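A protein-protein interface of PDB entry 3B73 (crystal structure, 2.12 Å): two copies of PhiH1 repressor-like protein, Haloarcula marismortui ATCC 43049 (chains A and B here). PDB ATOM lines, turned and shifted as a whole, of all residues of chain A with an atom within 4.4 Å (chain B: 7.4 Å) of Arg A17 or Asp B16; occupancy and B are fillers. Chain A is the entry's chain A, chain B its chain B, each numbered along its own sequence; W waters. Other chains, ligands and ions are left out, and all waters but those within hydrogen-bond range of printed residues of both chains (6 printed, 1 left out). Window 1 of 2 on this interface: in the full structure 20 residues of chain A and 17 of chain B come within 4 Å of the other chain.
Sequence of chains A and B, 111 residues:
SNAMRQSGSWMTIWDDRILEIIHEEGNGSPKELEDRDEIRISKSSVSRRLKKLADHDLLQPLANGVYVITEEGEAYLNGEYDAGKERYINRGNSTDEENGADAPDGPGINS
The guanidinium group (NH2) of Arg A17 is in salt-bridge range of the side-chain carboxylate (OD2) of Asp B16 (2.9 Å). OD2 of Asp A16 is in salt-bridge range of NH2 of Arg B17, at 2.6 Å. The side-chain hydroxyl of Ser B7 lies within hydrogen-bond range of the guanidinium group of Arg A17, 2.9 Å away.
NH1 of Arg B17 is in salt-bridge range of OE2 of Glu B20 (2.8 Å). The side-chain hydroxyl (OH) of Tyr B76 sits at hydrogen-bond distance from the side-chain hydroxyl (OG) of Ser B7 (2.8 Å). NH1 of Arg B5 lies within salt-bridge range of OE1 of Glu B20 (2.7 Å). The guanidinium group (NE) of Arg A17 is in salt-bridge range of the side-chain carboxylate (OE1) of Glu A20, 2.9 Å away. NH1 of Arg B5 lies within salt-bridge range of OD2 of Asp B16 (2.9 Å). OD1 of Asp B16 sits at hydrogen-bond distance from OH of Tyr B76 (2.7 Å).
Among the printed residues, merely in contact across the chains: Arg A5 with Arg B17 (3.6 Å), Ile A13 with Ser B7 (3.3 Å), Ile A13 with Met B11 (3.7 Å), Ile A13 with Thr B12 (3.5 Å), Ile A13 with Ile B13 (3.9 Å), Ile A13 with Asp B16 (3.5 Å), Ile A13 with Tyr B76 (3.8 Å), Trp A14 with Ser B7 (3.6 Å), Trp A14 with Gly B8 (3.7 Å), Asp A16 with Ile B13 (3.6 Å), Arg A17 with Arg B5 (3.4 Å), Arg A17 with Tyr B76 (3.7 Å), Glu A20 with Met B4 (3.9 Å) and Ile A21 with Met B4 (3.4 Å).
Arg A17 touches just these residues of chain B: Arg B5, Ser B7, Asp B16 and Tyr B76. Ile A18 touches none of the printed residues of chain B. Of the printed residues of chain B, Ile A21 touches Met B4. Printed residues of chain A within 4 Å of Ser B7: Ile A13 (3.3 Å), Trp A14 (3.6 Å) and Arg A17 (2.9 Å). Asp B16 touches just these residues of chain A: Ile A13 and Arg A17. Leu B53 touches none of the printed residues of chain A.
Of the 22 printed residues of chain B, 10 touch a printed residue of chain A. Hydrophobic or aromatic side chains of chain B that line the printed part of chain A: Met B4, Met B11, Ile B13 and Tyr B76. Printed residues of chain A that touch a printed residue of chain B: Arg A5, Ile A13, Trp A14, Asp A16, Arg A17, Glu A20 and Ile A21. Along chain A the printed residues that touch a printed residue of chain B span positions 5 to 21. Among the printed residues, 17 pairs touch across the chains.
Arg A5 touches Arg B17, and with the chains exchanged Arg A17 touches Arg B5. Ile A13 touches its own counterpart, Ile B13. Ile A13 touches Asp B16, and with the chains exchanged Asp A16 touches Ile B13. Asp A16 touches Arg B17, and with the chains exchanged Arg A17 touches Asp B16. Of the 17 pairs that touch across the chains among the printed residues, 7 have their exchanged pair printed and touching as well.
Water W6 lies within hydrogen-bond range of OE2 of Glu A20 (2.6 Å), NH1 of Arg A17 (3.4 Å) and NE of Arg B5 (3.4 Å). Water W5 bridges OE1 of Glu B20 (2.7 Å) and NE of Arg A5 (3.4 Å). Water W3 lies within hydrogen-bond range of the side-chain carboxylate of Glu B20 (2.7 Å) and the backbone NH of Arg A5 (2.9 Å). Water W1 bridges the side-chain carboxylate of Glu A20 (2.8 Å) and the backbone NH of Arg B5 (2.9 Å). Water W2 lies within hydrogen-bond range of the backbone carbonyl oxygen (O) of Met B11 (2.8 Å) and the backbone NH (N) of Ile A13 (3.0 Å). Water W4 bridges the backbone carbonyl oxygen of Arg A5 and the guanidinium group of Arg B17.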
ATOM      1  N   ARG A   5     -14.732 -27.330   6.241  1.00  0.00           N
ATOM      2  CA  ARG A   5     -14.001 -26.176   5.692  1.00  0.00           C
ATOM      3  C   ARG A   5     -12.484 -26.327   5.905  1.00  0.00           C
ATOM      4  O   ARG A   5     -12.021 -26.875   6.919  1.00  0.00           O
ATOM      5  CB  ARG A   5     -14.537 -24.833   6.257  1.00  0.00           C
ATOM      6  CG  ARG A   5     -15.527 -24.170   5.324  1.00  0.00           C
ATOM      7  CD  ARG A   5     -16.944 -24.166   5.822  1.00  0.00           C
ATOM      8  NE  ARG A   5     -17.070 -23.050   6.715  1.00  0.00           N
ATOM      9  CZ  ARG A   5     -18.169 -22.354   6.968  1.00  0.00           C
ATOM     10  NH1 ARG A   5     -19.341 -22.617   6.403  1.00  0.00           N
ATOM     11  NH2 ARG A   5     -18.060 -21.364   7.824  1.00  0.00           N
ATOM     12  N   ILE A  13     -12.324 -15.915  13.048  1.00  0.00           N
ATOM     13  CA  ILE A  13     -13.633 -16.539  13.120  1.00  0.00           C
ATOM     14  C   ILE A  13     -14.665 -15.665  12.373  1.00  0.00           C
ATOM     15  O   ILE A  13     -15.545 -16.169  11.695  1.00  0.00           O
ATOM     16  CB  ILE A  13     -14.016 -16.829  14.576  1.00  0.00           C
ATOM     17  CG1 ILE A  13     -15.281 -17.694  14.637  1.00  0.00           C
ATOM     18  CG2 ILE A  13     -14.141 -15.509  15.402  1.00  0.00           C
ATOM     19  CD1 ILE A  13     -15.267 -18.650  15.768  1.00  0.00           C
ATOM     20  N   TRP A  14     -14.488 -14.350  12.463  1.00  0.00           N
ATOM     21  CA  TRP A  14     -15.381 -13.388  11.851  1.00  0.00           C
ATOM     22  C   TRP A  14     -15.374 -13.476  10.352  1.00  0.00           C
ATOM     23  O   TRP A  14     -16.359 -13.126   9.726  1.00  0.00           O
ATOM     24  CB  TRP A  14     -15.025 -11.964  12.320  1.00  0.00           C
ATOM     25  CG  TRP A  14     -14.995 -11.970  13.794  1.00  0.00           C
ATOM     26  CD1 TRP A  14     -13.898 -11.839  14.602  1.00  0.00           C
ATOM     27  CD2 TRP A  14     -16.104 -12.247  14.654  1.00  0.00           C
ATOM     28  NE1 TRP A  14     -14.270 -11.981  15.927  1.00  0.00           N
ATOM     29  CE2 TRP A  14     -15.617 -12.225  15.982  1.00  0.00           C
ATOM     30  CE3 TRP A  14     -17.464 -12.516  14.431  1.00  0.00           C
ATOM     31  CZ2 TRP A  14     -16.441 -12.451  17.076  1.00  0.00           C
ATOM     32  CZ3 TRP A  14     -18.285 -12.757  15.530  1.00  0.00           C
ATOM     33  CH2 TRP A  14     -17.772 -12.706  16.834  1.00  0.00           C
ATOM     34  N   ASP A  15     -14.273 -13.947   9.770  1.00  0.00           N
ATOM     35  CA  ASP A  15     -14.272 -14.191   8.329  1.00  0.00           C
ATOM     36  C   ASP A  15     -15.354 -15.204   7.948  1.00  0.00           C
ATOM     37  O   ASP A  15     -16.045 -15.005   6.970  1.00  0.00           O
ATOM     38  CB  ASP A  15     -12.925 -14.703   7.845  1.00  0.00           C
ATOM     39  CG  ASP A  15     -11.821 -13.678   8.001  1.00  0.00           C
ATOM     40  OD1 ASP A  15     -12.139 -12.479   8.073  1.00  0.00           O
ATOM     41  OD2 ASP A  15     -10.633 -14.067   8.063  1.00  0.00           O
ATOM     42  N   ASP A  16     -15.510 -16.285   8.710  1.00  0.00           N
ATOM     43  CA  ASP A  16     -16.528 -17.282   8.350  1.00  0.00           C
ATOM     44  C   ASP A  16     -17.896 -16.672   8.527  1.00  0.00           C
ATOM     45  O   ASP A  16     -18.763 -16.814   7.655  1.00  0.00           O
ATOM     46  CB  ASP A  16     -16.453 -18.563   9.214  1.00  0.00           C
ATOM     47  CG  ASP A  16     -15.493 -19.638   8.649  1.00  0.00           C
ATOM     48  OD1 ASP A  16     -14.741 -19.400   7.682  1.00  0.00           O
ATOM     49  OD2 ASP A  16     -15.492 -20.751   9.207  1.00  0.00           O
ATOM     50  N   ARG A  17     -18.092 -15.994   9.661  1.00  0.00           N
ATOM     51  CA  ARG A  17     -19.398 -15.389   9.931  1.00  0.00           C
ATOM     52  C   ARG A  17     -19.735 -14.409   8.816  1.00  0.00           C
ATOM     53  O   ARG A  17     -20.874 -14.345   8.323  1.00  0.00           O
ATOM     54  CB  ARG A  17     -19.444 -14.653  11.276  1.00  0.00           C
ATOM     55  CG  ARG A  17     -19.086 -15.444  12.515  1.00  0.00           C
ATOM     56  CD  ARG A  17     -20.076 -16.601  12.904  1.00  0.00           C
ATOM     57  NE  ARG A  17     -19.899 -17.759  12.046  1.00  0.00           N
ATOM     58  CZ  ARG A  17     -19.102 -18.781  12.324  1.00  0.00           C
ATOM     59  NH1 ARG A  17     -19.017 -19.783  11.454  1.00  0.00           N
ATOM     60  NH2 ARG A  17     -18.405 -18.818  13.470  1.00  0.00           N
ATOM     61  N   ILE A  18     -18.734 -13.640   8.411  1.00  0.00           N
ATOM     62  CA  ILE A  18     -18.941 -12.623   7.392  1.00  0.00           C
ATOM     63  C   ILE A  18     -19.253 -13.233   6.045  1.00  0.00           C
ATOM     64  O   ILE A  18     -20.120 -12.747   5.318  1.00  0.00           O
ATOM     65  CB  ILE A  18     -17.705 -11.746   7.240  1.00  0.00           C
ATOM     66  CG1 ILE A  18     -17.638 -10.729   8.373  1.00  0.00           C
ATOM     67  CG2 ILE A  18     -17.730 -11.030   5.938  1.00  0.00           C
ATOM     68  CD1 ILE A  18     -16.323  -9.947   8.405  1.00  0.00           C
ATOM     69  N   LEU A  19     -18.517 -14.280   5.690  1.00  0.00           N
ATOM     70  CA  LEU A  19     -18.754 -14.956   4.424  1.00  0.00           C
ATOM     71  C   LEU A  19     -20.150 -15.563   4.445  1.00  0.00           C
ATOM     72  O   LEU A  19     -20.883 -15.469   3.466  1.00  0.00           O
ATOM     73  CB  LEU A  19     -17.712 -16.047   4.173  1.00  0.00           C
ATOM     74  CG  LEU A  19     -16.359 -15.587   3.634  1.00  0.00           C
ATOM     75  CD1 LEU A  19     -15.396 -16.750   3.637  1.00  0.00           C
ATOM     76  CD2 LEU A  19     -16.498 -15.020   2.211  1.00  0.00           C
ATOM     77  N   GLU A  20     -20.514 -16.154   5.582  1.00  0.00           N
ATOM     78  CA  GLU A  20     -21.815 -16.805   5.727  1.00  0.00           C
ATOM     79  C   GLU A  20     -22.939 -15.801   5.565  1.00  0.00           C
ATOM     80  O   GLU A  20     -23.922 -16.092   4.898  1.00  0.00           O
ATOM     81  CB  GLU A  20     -21.958 -17.496   7.093  1.00  0.00           C
ATOM     82  CG  GLU A  20     -21.153 -18.776   7.194  1.00  0.00           C
ATOM     83  CD  GLU A  20     -20.978 -19.229   8.643  1.00  0.00           C
ATOM     84  OE1 GLU A  20     -21.321 -18.473   9.580  1.00  0.00           O
ATOM     85  OE2 GLU A  20     -20.486 -20.349   8.850  1.00  0.00           O
ATOM     86  N   ILE A  21     -22.806 -14.629   6.187  1.00  0.00           N
ATOM     87  CA  ILE A  21     -23.852 -13.625   6.066  1.00  0.00           C
ATOM     88  C   ILE A  21     -23.964 -13.145   4.626  1.00  0.00           C
ATOM     89  O   ILE A  21     -25.050 -13.119   4.060  1.00  0.00           O
ATOM     90  CB  ILE A  21     -23.624 -12.416   6.966  1.00  0.00           C
ATOM     91  CG1 ILE A  21     -23.837 -12.784   8.441  1.00  0.00           C
ATOM     92  CG2 ILE A  21     -24.584 -11.264   6.570  1.00  0.00           C
ATOM     93  CD1 ILE A  21     -23.296 -11.709   9.388  1.00  0.00           C
ATOM     94  N   ILE A  39     -22.084 -10.370  14.563  1.00  0.00           N
ATOM     95  CA  ILE A  39     -20.768  -9.796  14.319  1.00  0.00           C
ATOM     96  C   ILE A  39     -20.315  -8.988  15.519  1.00  0.00           C
ATOM     97  O   ILE A  39     -20.889  -7.946  15.825  1.00  0.00           O
ATOM     98  CB  ILE A  39     -20.761  -8.930  13.041  1.00  0.00           C
ATOM     99  CG1 ILE A  39     -21.226  -9.773  11.849  1.00  0.00           C
ATOM    100  CG2 ILE A  39     -19.347  -8.356  12.779  1.00  0.00           C
ATOM    101  CD1 ILE A  39     -20.279 -10.916  11.494  1.00  0.00           C
ATOM    102  N   MET B   4     -27.416 -19.262  12.112  1.00  0.00           N
ATOM    103  CA  MET B   4     -26.000 -18.912  12.093  1.00  0.00           C
ATOM    104  C   MET B   4     -25.363 -18.932  13.487  1.00  0.00           C
ATOM    105  O   MET B   4     -25.972 -18.502  14.470  1.00  0.00           O
ATOM    106  CB  MET B   4     -25.839 -17.524  11.501  1.00  0.00           C
ATOM    107  CG  MET B   4     -24.430 -17.041  11.494  1.00  0.00           C
ATOM    108  SD  MET B   4     -24.439 -15.569  10.294  1.00  0.00           S
ATOM    109  CE  MET B   4     -25.466 -16.397   8.860  1.00  0.00           C
ATOM    110  N   ARG B   5     -24.130 -19.416  13.569  1.00  0.00           N
ATOM    111  CA  ARG B   5     -23.381 -19.414  14.833  1.00  0.00           C
ATOM    112  C   ARG B   5     -23.216 -18.019  15.447  1.00  0.00           C
ATOM    113  O   ARG B   5     -22.945 -17.039  14.738  1.00  0.00           O
ATOM    114  CB  ARG B   5     -22.008 -20.055  14.625  1.00  0.00           C
ATOM    115  CG  ARG B   5     -22.119 -21.546  14.484  1.00  0.00           C
ATOM    116  CD  ARG B   5     -20.816 -22.147  14.085  1.00  0.00           C
ATOM    117  NE  ARG B   5     -21.027 -23.483  13.555  1.00  0.00           N
ATOM    118  CZ  ARG B   5     -20.057 -24.226  13.041  1.00  0.00           C
ATOM    119  NH1 ARG B   5     -18.805 -23.768  13.000  1.00  0.00           N
ATOM    120  NH2 ARG B   5     -20.335 -25.429  12.576  1.00  0.00           N
ATOM    121  N   GLN B   6     -23.408 -17.939  16.763  1.00  0.00           N
ATOM    122  CA  GLN B   6     -23.191 -16.702  17.507  1.00  0.00           C
ATOM    123  C   GLN B   6     -21.851 -16.835  18.211  1.00  0.00           C
ATOM    124  O   GLN B   6     -21.813 -17.300  19.351  1.00  0.00           O
ATOM    125  CB  GLN B   6     -24.261 -16.543  18.597  1.00  0.00           C
ATOM    126  CG  GLN B   6     -25.374 -15.623  18.275  1.00  0.00           C
ATOM    127  CD  GLN B   6     -24.899 -14.240  17.901  1.00  0.00           C
ATOM    128  OE1 GLN B   6     -25.494 -13.627  17.042  1.00  0.00           O
ATOM    129  NE2 GLN B   6     -23.817 -13.744  18.537  1.00  0.00           N
ATOM    130  N   SER B   7     -20.765 -16.445  17.551  1.00  0.00           N
ATOM    131  CA  SER B   7     -19.423 -16.633  18.127  1.00  0.00           C
ATOM    132  C   SER B   7     -19.100 -15.614  19.220  1.00  0.00           C
ATOM    133  O   SER B   7     -19.711 -14.554  19.293  1.00  0.00           O
ATOM    134  CB  SER B   7     -18.352 -16.531  17.043  1.00  0.00           C
ATOM    135  OG  SER B   7     -18.428 -17.612  16.134  1.00  0.00           O
ATOM    136  N   GLY B   8     -18.132 -15.956  20.058  1.00  0.00           N
ATOM    137  CA  GLY B   8     -17.645 -15.068  21.095  1.00  0.00           C
ATOM    138  C   GLY B   8     -16.379 -14.362  20.646  1.00  0.00           C
ATOM    139  O   GLY B   8     -15.641 -14.864  19.796  1.00  0.00           O
ATOM    140  N   MET B  11     -12.924 -16.113  20.496  1.00  0.00           N
ATOM    141  CA  MET B  11     -12.716 -17.304  19.677  1.00  0.00           C
ATOM    142  C   MET B  11     -11.792 -17.048  18.504  1.00  0.00           C
ATOM    143  O   MET B  11     -11.640 -15.917  18.051  1.00  0.00           O
ATOM    144  CB  MET B  11     -14.045 -17.892  19.183  1.00  0.00           C
ATOM    145  CG  MET B  11     -14.957 -18.382  20.276  1.00  0.00           C
ATOM    146  SD  MET B  11     -16.589 -19.119  19.507  1.00  0.00           S
ATOM    147  CE  MET B  11     -15.858 -20.732  18.844  1.00  0.00           C
ATOM    148  N   THR B  12     -11.166 -18.122  18.029  1.00  0.00           N
ATOM    149  CA  THR B  12     -10.393 -18.111  16.802  1.00  0.00           C
ATOM    150  C   THR B  12     -11.080 -19.047  15.833  1.00  0.00           C
ATOM    151  O   THR B  12     -11.982 -19.800  16.192  1.00  0.00           O
ATOM    152  CB  THR B  12      -8.964 -18.657  17.026  1.00  0.00           C
ATOM    153  OG1 THR B  12      -9.031 -20.051  17.374  1.00  0.00           O
ATOM    154  CG2 THR B  12      -8.272 -17.885  18.153  1.00  0.00           C
ATOM    155  N   ILE B  13     -10.636 -19.047  14.600  1.00  0.00           N
ATOM    156  CA  ILE B  13     -11.327 -19.865  13.617  1.00  0.00           C
ATOM    157  C   ILE B  13     -11.095 -21.348  13.910  1.00  0.00           C
ATOM    158  O   ILE B  13     -11.930 -22.189  13.574  1.00  0.00           O
ATOM    159  CB  ILE B  13     -10.930 -19.461  12.175  1.00  0.00           C
ATOM    160  CG1 ILE B  13     -11.878 -20.111  11.166  1.00  0.00           C
ATOM    161  CG2 ILE B  13      -9.480 -19.798  11.919  1.00  0.00           C
ATOM    162  CD1 ILE B  13     -11.861 -19.501   9.838  1.00  0.00           C
ATOM    163  N   TRP B  14      -9.979 -21.654  14.581  1.00  0.00           N
ATOM    164  CA  TRP B  14      -9.580 -23.029  14.842  1.00  0.00           C
ATOM    165  C   TRP B  14     -10.459 -23.644  15.905  1.00  0.00           C
ATOM    166  O   TRP B  14     -10.634 -24.858  15.952  1.00  0.00           O
ATOM    167  CB  TRP B  14      -8.078 -23.113  15.188  1.00  0.00           C
ATOM    168  CG  TRP B  14      -7.288 -22.435  14.097  1.00  0.00           C
ATOM    169  CD1 TRP B  14      -6.620 -21.244  14.183  1.00  0.00           C
ATOM    170  CD2 TRP B  14      -7.188 -22.855  12.719  1.00  0.00           C
ATOM    171  NE1 TRP B  14      -6.087 -20.917  12.946  1.00  0.00           N
ATOM    172  CE2 TRP B  14      -6.416 -21.892  12.040  1.00  0.00           C
ATOM    173  CE3 TRP B  14      -7.647 -23.967  12.010  1.00  0.00           C
ATOM    174  CZ2 TRP B  14      -6.099 -22.005  10.678  1.00  0.00           C
ATOM    175  CZ3 TRP B  14      -7.342 -24.068  10.659  1.00  0.00           C
ATOM    176  CH2 TRP B  14      -6.573 -23.092  10.012  1.00  0.00           C
ATOM    177  N   ASP B  15     -11.030 -22.792  16.741  1.00  0.00           N
ATOM    178  CA  ASP B  15     -12.073 -23.210  17.665  1.00  0.00           C
ATOM    179  C   ASP B  15     -13.250 -23.925  16.976  1.00  0.00           C
ATOM    180  O   ASP B  15     -13.703 -24.960  17.471  1.00  0.00           O
ATOM    181  CB  ASP B  15     -12.576 -22.008  18.472  1.00  0.00           C
ATOM    182  CG  ASP B  15     -11.512 -21.469  19.418  1.00  0.00           C
ATOM    183  OD1 ASP B  15     -10.552 -22.221  19.720  1.00  0.00           O
ATOM    184  OD2 ASP B  15     -11.619 -20.296  19.834  1.00  0.00           O
ATOM    185  N   ASP B  16     -13.744 -23.371  15.867  1.00  0.00           N
ATOM    186  CA  ASP B  16     -14.885 -23.962  15.167  1.00  0.00           C
ATOM    187  C   ASP B  16     -14.435 -25.288  14.583  1.00  0.00           C
ATOM    188  O   ASP B  16     -15.156 -26.291  14.662  1.00  0.00           O
ATOM    189  CB  ASP B  16     -15.416 -23.049  14.040  1.00  0.00           C
ATOM    190  CG  ASP B  16     -16.488 -22.064  14.523  1.00  0.00           C
ATOM    191  OD1 ASP B  16     -16.641 -21.859  15.743  1.00  0.00           O
ATOM    192  OD2 ASP B  16     -17.169 -21.462  13.678  1.00  0.00           O
ATOM    193  N   ARG B  17     -13.228 -25.293  14.027  1.00  0.00           N
ATOM    194  CA  ARG B  17     -12.672 -26.512  13.449  1.00  0.00           C
ATOM    195  C   ARG B  17     -12.537 -27.587  14.502  1.00  0.00           C
ATOM    196  O   ARG B  17     -12.992 -28.715  14.315  1.00  0.00           O
ATOM    197  CB  ARG B  17     -11.313 -26.261  12.796  1.00  0.00           C
ATOM    198  CG  ARG B  17     -11.372 -25.297  11.642  1.00  0.00           C
ATOM    199  CD  ARG B  17     -12.371 -25.737  10.581  1.00  0.00           C
ATOM    200  NE  ARG B  17     -12.668 -24.568   9.789  1.00  0.00           N
ATOM    201  CZ  ARG B  17     -13.809 -23.900   9.842  1.00  0.00           C
ATOM    202  NH1 ARG B  17     -14.815 -24.331  10.582  1.00  0.00           N
ATOM    203  NH2 ARG B  17     -13.945 -22.811   9.118  1.00  0.00           N
ATOM    204  N   ILE B  18     -11.936 -27.240  15.633  1.00  0.00           N
ATOM    205  CA  ILE B  18     -11.797 -28.228  16.686  1.00  0.00           C
ATOM    206  C   ILE B  18     -13.164 -28.725  17.127  1.00  0.00           C
ATOM    207  O   ILE B  18     -13.361 -29.922  17.269  1.00  0.00           O
ATOM    208  CB  ILE B  18     -11.042 -27.670  17.875  1.00  0.00           C
ATOM    209  CG1 ILE B  18      -9.596 -27.383  17.464  1.00  0.00           C
ATOM    210  CG2 ILE B  18     -11.150 -28.629  19.050  1.00  0.00           C
ATOM    211  CD1 ILE B  18      -8.907 -26.468  18.381  1.00  0.00           C
ATOM    212  N   LEU B  19     -14.115 -27.817  17.345  1.00  0.00           N
ATOM    213  CA  LEU B  19     -15.440 -28.269  17.770  1.00  0.00           C
ATOM    214  C   LEU B  19     -16.070 -29.214  16.744  1.00  0.00           C
ATOM    215  O   LEU B  19     -16.647 -30.233  17.105  1.00  0.00           O
ATOM    216  CB  LEU B  19     -16.375 -27.094  18.061  1.00  0.00           C
ATOM    217  CG  LEU B  19     -16.120 -26.401  19.390  1.00  0.00           C
ATOM    218  CD1 LEU B  19     -16.867 -25.096  19.416  1.00  0.00           C
ATOM    219  CD2 LEU B  19     -16.517 -27.305  20.583  1.00  0.00           C
ATOM    220  N   GLU B  20     -15.934 -28.877  15.466  1.00  0.00           N
ATOM    221  CA  GLU B  20     -16.508 -29.662  14.371  1.00  0.00           C
ATOM    222  C   GLU B  20     -15.884 -31.056  14.312  1.00  0.00           C
ATOM    223  O   GLU B  20     -16.569 -32.051  14.080  1.00  0.00           O
ATOM    224  CB  GLU B  20     -16.329 -28.933  13.028  1.00  0.00           C
ATOM    225  CG  GLU B  20     -17.219 -27.688  12.915  1.00  0.00           C
ATOM    226  CD  GLU B  20     -16.774 -26.706  11.835  1.00  0.00           C
ATOM    227  OE1 GLU B  20     -17.510 -25.723  11.624  1.00  0.00           O
ATOM    228  OE2 GLU B  20     -15.706 -26.900  11.199  1.00  0.00           O
ATOM    229  N   ILE B  21     -14.584 -31.125  14.550  1.00  0.00           N
ATOM    230  CA  ILE B  21     -13.890 -32.397  14.490  1.00  0.00           C
ATOM    231  C   ILE B  21     -14.285 -33.272  15.664  1.00  0.00           C
ATOM    232  O   ILE B  21     -14.559 -34.461  15.505  1.00  0.00           O
ATOM    233  CB  ILE B  21     -12.364 -32.212  14.440  1.00  0.00           C
ATOM    234  CG1 ILE B  21     -11.943 -31.807  13.022  1.00  0.00           C
ATOM    235  CG2 ILE B  21     -11.663 -33.498  14.848  1.00  0.00           C
ATOM    236  CD1 ILE B  21     -10.564 -31.116  12.956  1.00  0.00           C
ATOM    237  N   ILE B  22     -14.331 -32.693  16.849  1.00  0.00           N
ATOM    238  CA  ILE B  22     -14.706 -33.481  18.006  1.00  0.00           C
ATOM    239  C   ILE B  22     -16.181 -33.910  17.903  1.00  0.00           C
ATOM    240  O   ILE B  22     -16.531 -35.019  18.271  1.00  0.00           O
ATOM    241  CB  ILE B  22     -14.419 -32.719  19.304  1.00  0.00           C
ATOM    242  CG1 ILE B  22     -12.901 -32.570  19.475  1.00  0.00           C
ATOM    243  CG2 ILE B  22     -15.053 -33.434  20.503  1.00  0.00           C
ATOM    244  CD1 ILE B  22     -12.504 -31.855  20.751  1.00  0.00           C
ATOM    245  N   ILE B  39      -6.571 -28.679  10.493  1.00  0.00           N
ATOM    246  CA  ILE B  39      -5.973 -27.938  11.595  1.00  0.00           C
ATOM    247  C   ILE B  39      -4.609 -27.418  11.159  1.00  0.00           C
ATOM    248  O   ILE B  39      -3.716 -28.204  10.861  1.00  0.00           O
ATOM    249  CB  ILE B  39      -5.842 -28.806  12.849  1.00  0.00           C
ATOM    250  CG1 ILE B  39      -7.219 -29.342  13.286  1.00  0.00           C
ATOM    251  CG2 ILE B  39      -5.154 -28.028  13.984  1.00  0.00           C
ATOM    252  CD1 ILE B  39      -8.309 -28.278  13.437  1.00  0.00           C
ATOM    253  N   LEU B  53     -11.720 -23.762  25.109  1.00  0.00           N
ATOM    254  CA  LEU B  53     -13.050 -24.284  24.852  1.00  0.00           C
ATOM    255  C   LEU B  53     -13.644 -24.930  26.102  1.00  0.00           C
ATOM    256  O   LEU B  53     -14.848 -24.795  26.355  1.00  0.00           O
ATOM    257  CB  LEU B  53     -13.021 -25.257  23.661  1.00  0.00           C
ATOM    258  CG  LEU B  53     -12.739 -24.513  22.348  1.00  0.00           C
ATOM    259  CD1 LEU B  53     -12.116 -25.405  21.273  1.00  0.00           C
ATOM    260  CD2 LEU B  53     -13.983 -23.790  21.868  1.00  0.00           C
ATOM    261  N   LEU B  58     -17.675 -25.448  26.244  1.00  0.00           N
ATOM    262  CA  LEU B  58     -18.020 -25.972  24.937  1.00  0.00           C
ATOM    263  C   LEU B  58     -17.429 -27.365  24.771  1.00  0.00           C
ATOM    264  O   LEU B  58     -17.897 -28.165  23.947  1.00  0.00           O
ATOM    265  CB  LEU B  58     -17.499 -25.033  23.863  1.00  0.00           C
ATOM    266  CG  LEU B  58     -18.116 -23.641  23.985  1.00  0.00           C
ATOM    267  CD1 LEU B  58     -17.790 -22.773  22.762  1.00  0.00           C
ATOM    268  CD2 LEU B  58     -19.635 -23.730  24.192  1.00  0.00           C
ATOM    269  N   TYR B  76     -24.046 -24.619  20.289  1.00  0.00           N
ATOM    270  CA  TYR B  76     -23.284 -23.521  19.666  1.00  0.00           C
ATOM    271  C   TYR B  76     -23.078 -23.770  18.161  1.00  0.00           C
ATOM    272  O   TYR B  76     -23.347 -22.898  17.332  1.00  0.00           O
ATOM    273  CB  TYR B  76     -21.920 -23.302  20.355  1.00  0.00           C
ATOM    274  CG  TYR B  76     -20.981 -22.517  19.455  1.00  0.00           C
ATOM    275  CD1 TYR B  76     -21.158 -21.138  19.278  1.00  0.00           C
ATOM    276  CD2 TYR B  76     -19.948 -23.158  18.740  1.00  0.00           C
ATOM    277  CE1 TYR B  76     -20.322 -20.397  18.416  1.00  0.00           C
ATOM    278  CE2 TYR B  76     -19.098 -22.419  17.883  1.00  0.00           C
ATOM    279  CZ  TYR B  76     -19.289 -21.035  17.742  1.00  0.00           C
ATOM    280  OH  TYR B  76     -18.497 -20.288  16.891  1.00  0.00           O
ATOM    281  N   LEU B  77     -22.579 -24.956  17.810  1.00  0.00           N
ATOM    282  CA  LEU B  77     -22.418 -25.302  16.390  1.00  0.00           C
ATOM    283  C   LEU B  77     -23.731 -25.112  15.592  1.00  0.00           C
ATOM    284  O   LEU B  77     -23.700 -24.757  14.405  1.00  0.00           O
ATOM    285  CB  LEU B  77     -21.894 -26.738  16.241  1.00  0.00           C
ATOM    286  CG  LEU B  77     -20.505 -26.995  16.843  1.00  0.00           C
ATOM    287  CD1 LEU B  77     -20.114 -28.460  16.772  1.00  0.00           C
ATOM    288  CD2 LEU B  77     -19.439 -26.147  16.154  1.00  0.00           C
HETATM  289  O   HOH W   1     -22.964 -20.239  11.036  1.00  0.00           O
HETATM  290  O   HOH W   2     -10.853 -14.994  15.506  1.00  0.00           O
HETATM  291  O   HOH W   3     -16.433 -26.844   8.571  1.00  0.00           O
HETATM  292  O   HOH W   4      -9.873 -25.620   8.375  1.00  0.00           O
HETATM  293  O   HOH W   5     -18.518 -24.435   9.500  1.00  0.00           O
HETATM  294  O   HOH W   6     -20.735 -22.461  10.300  1.00  0.00           O
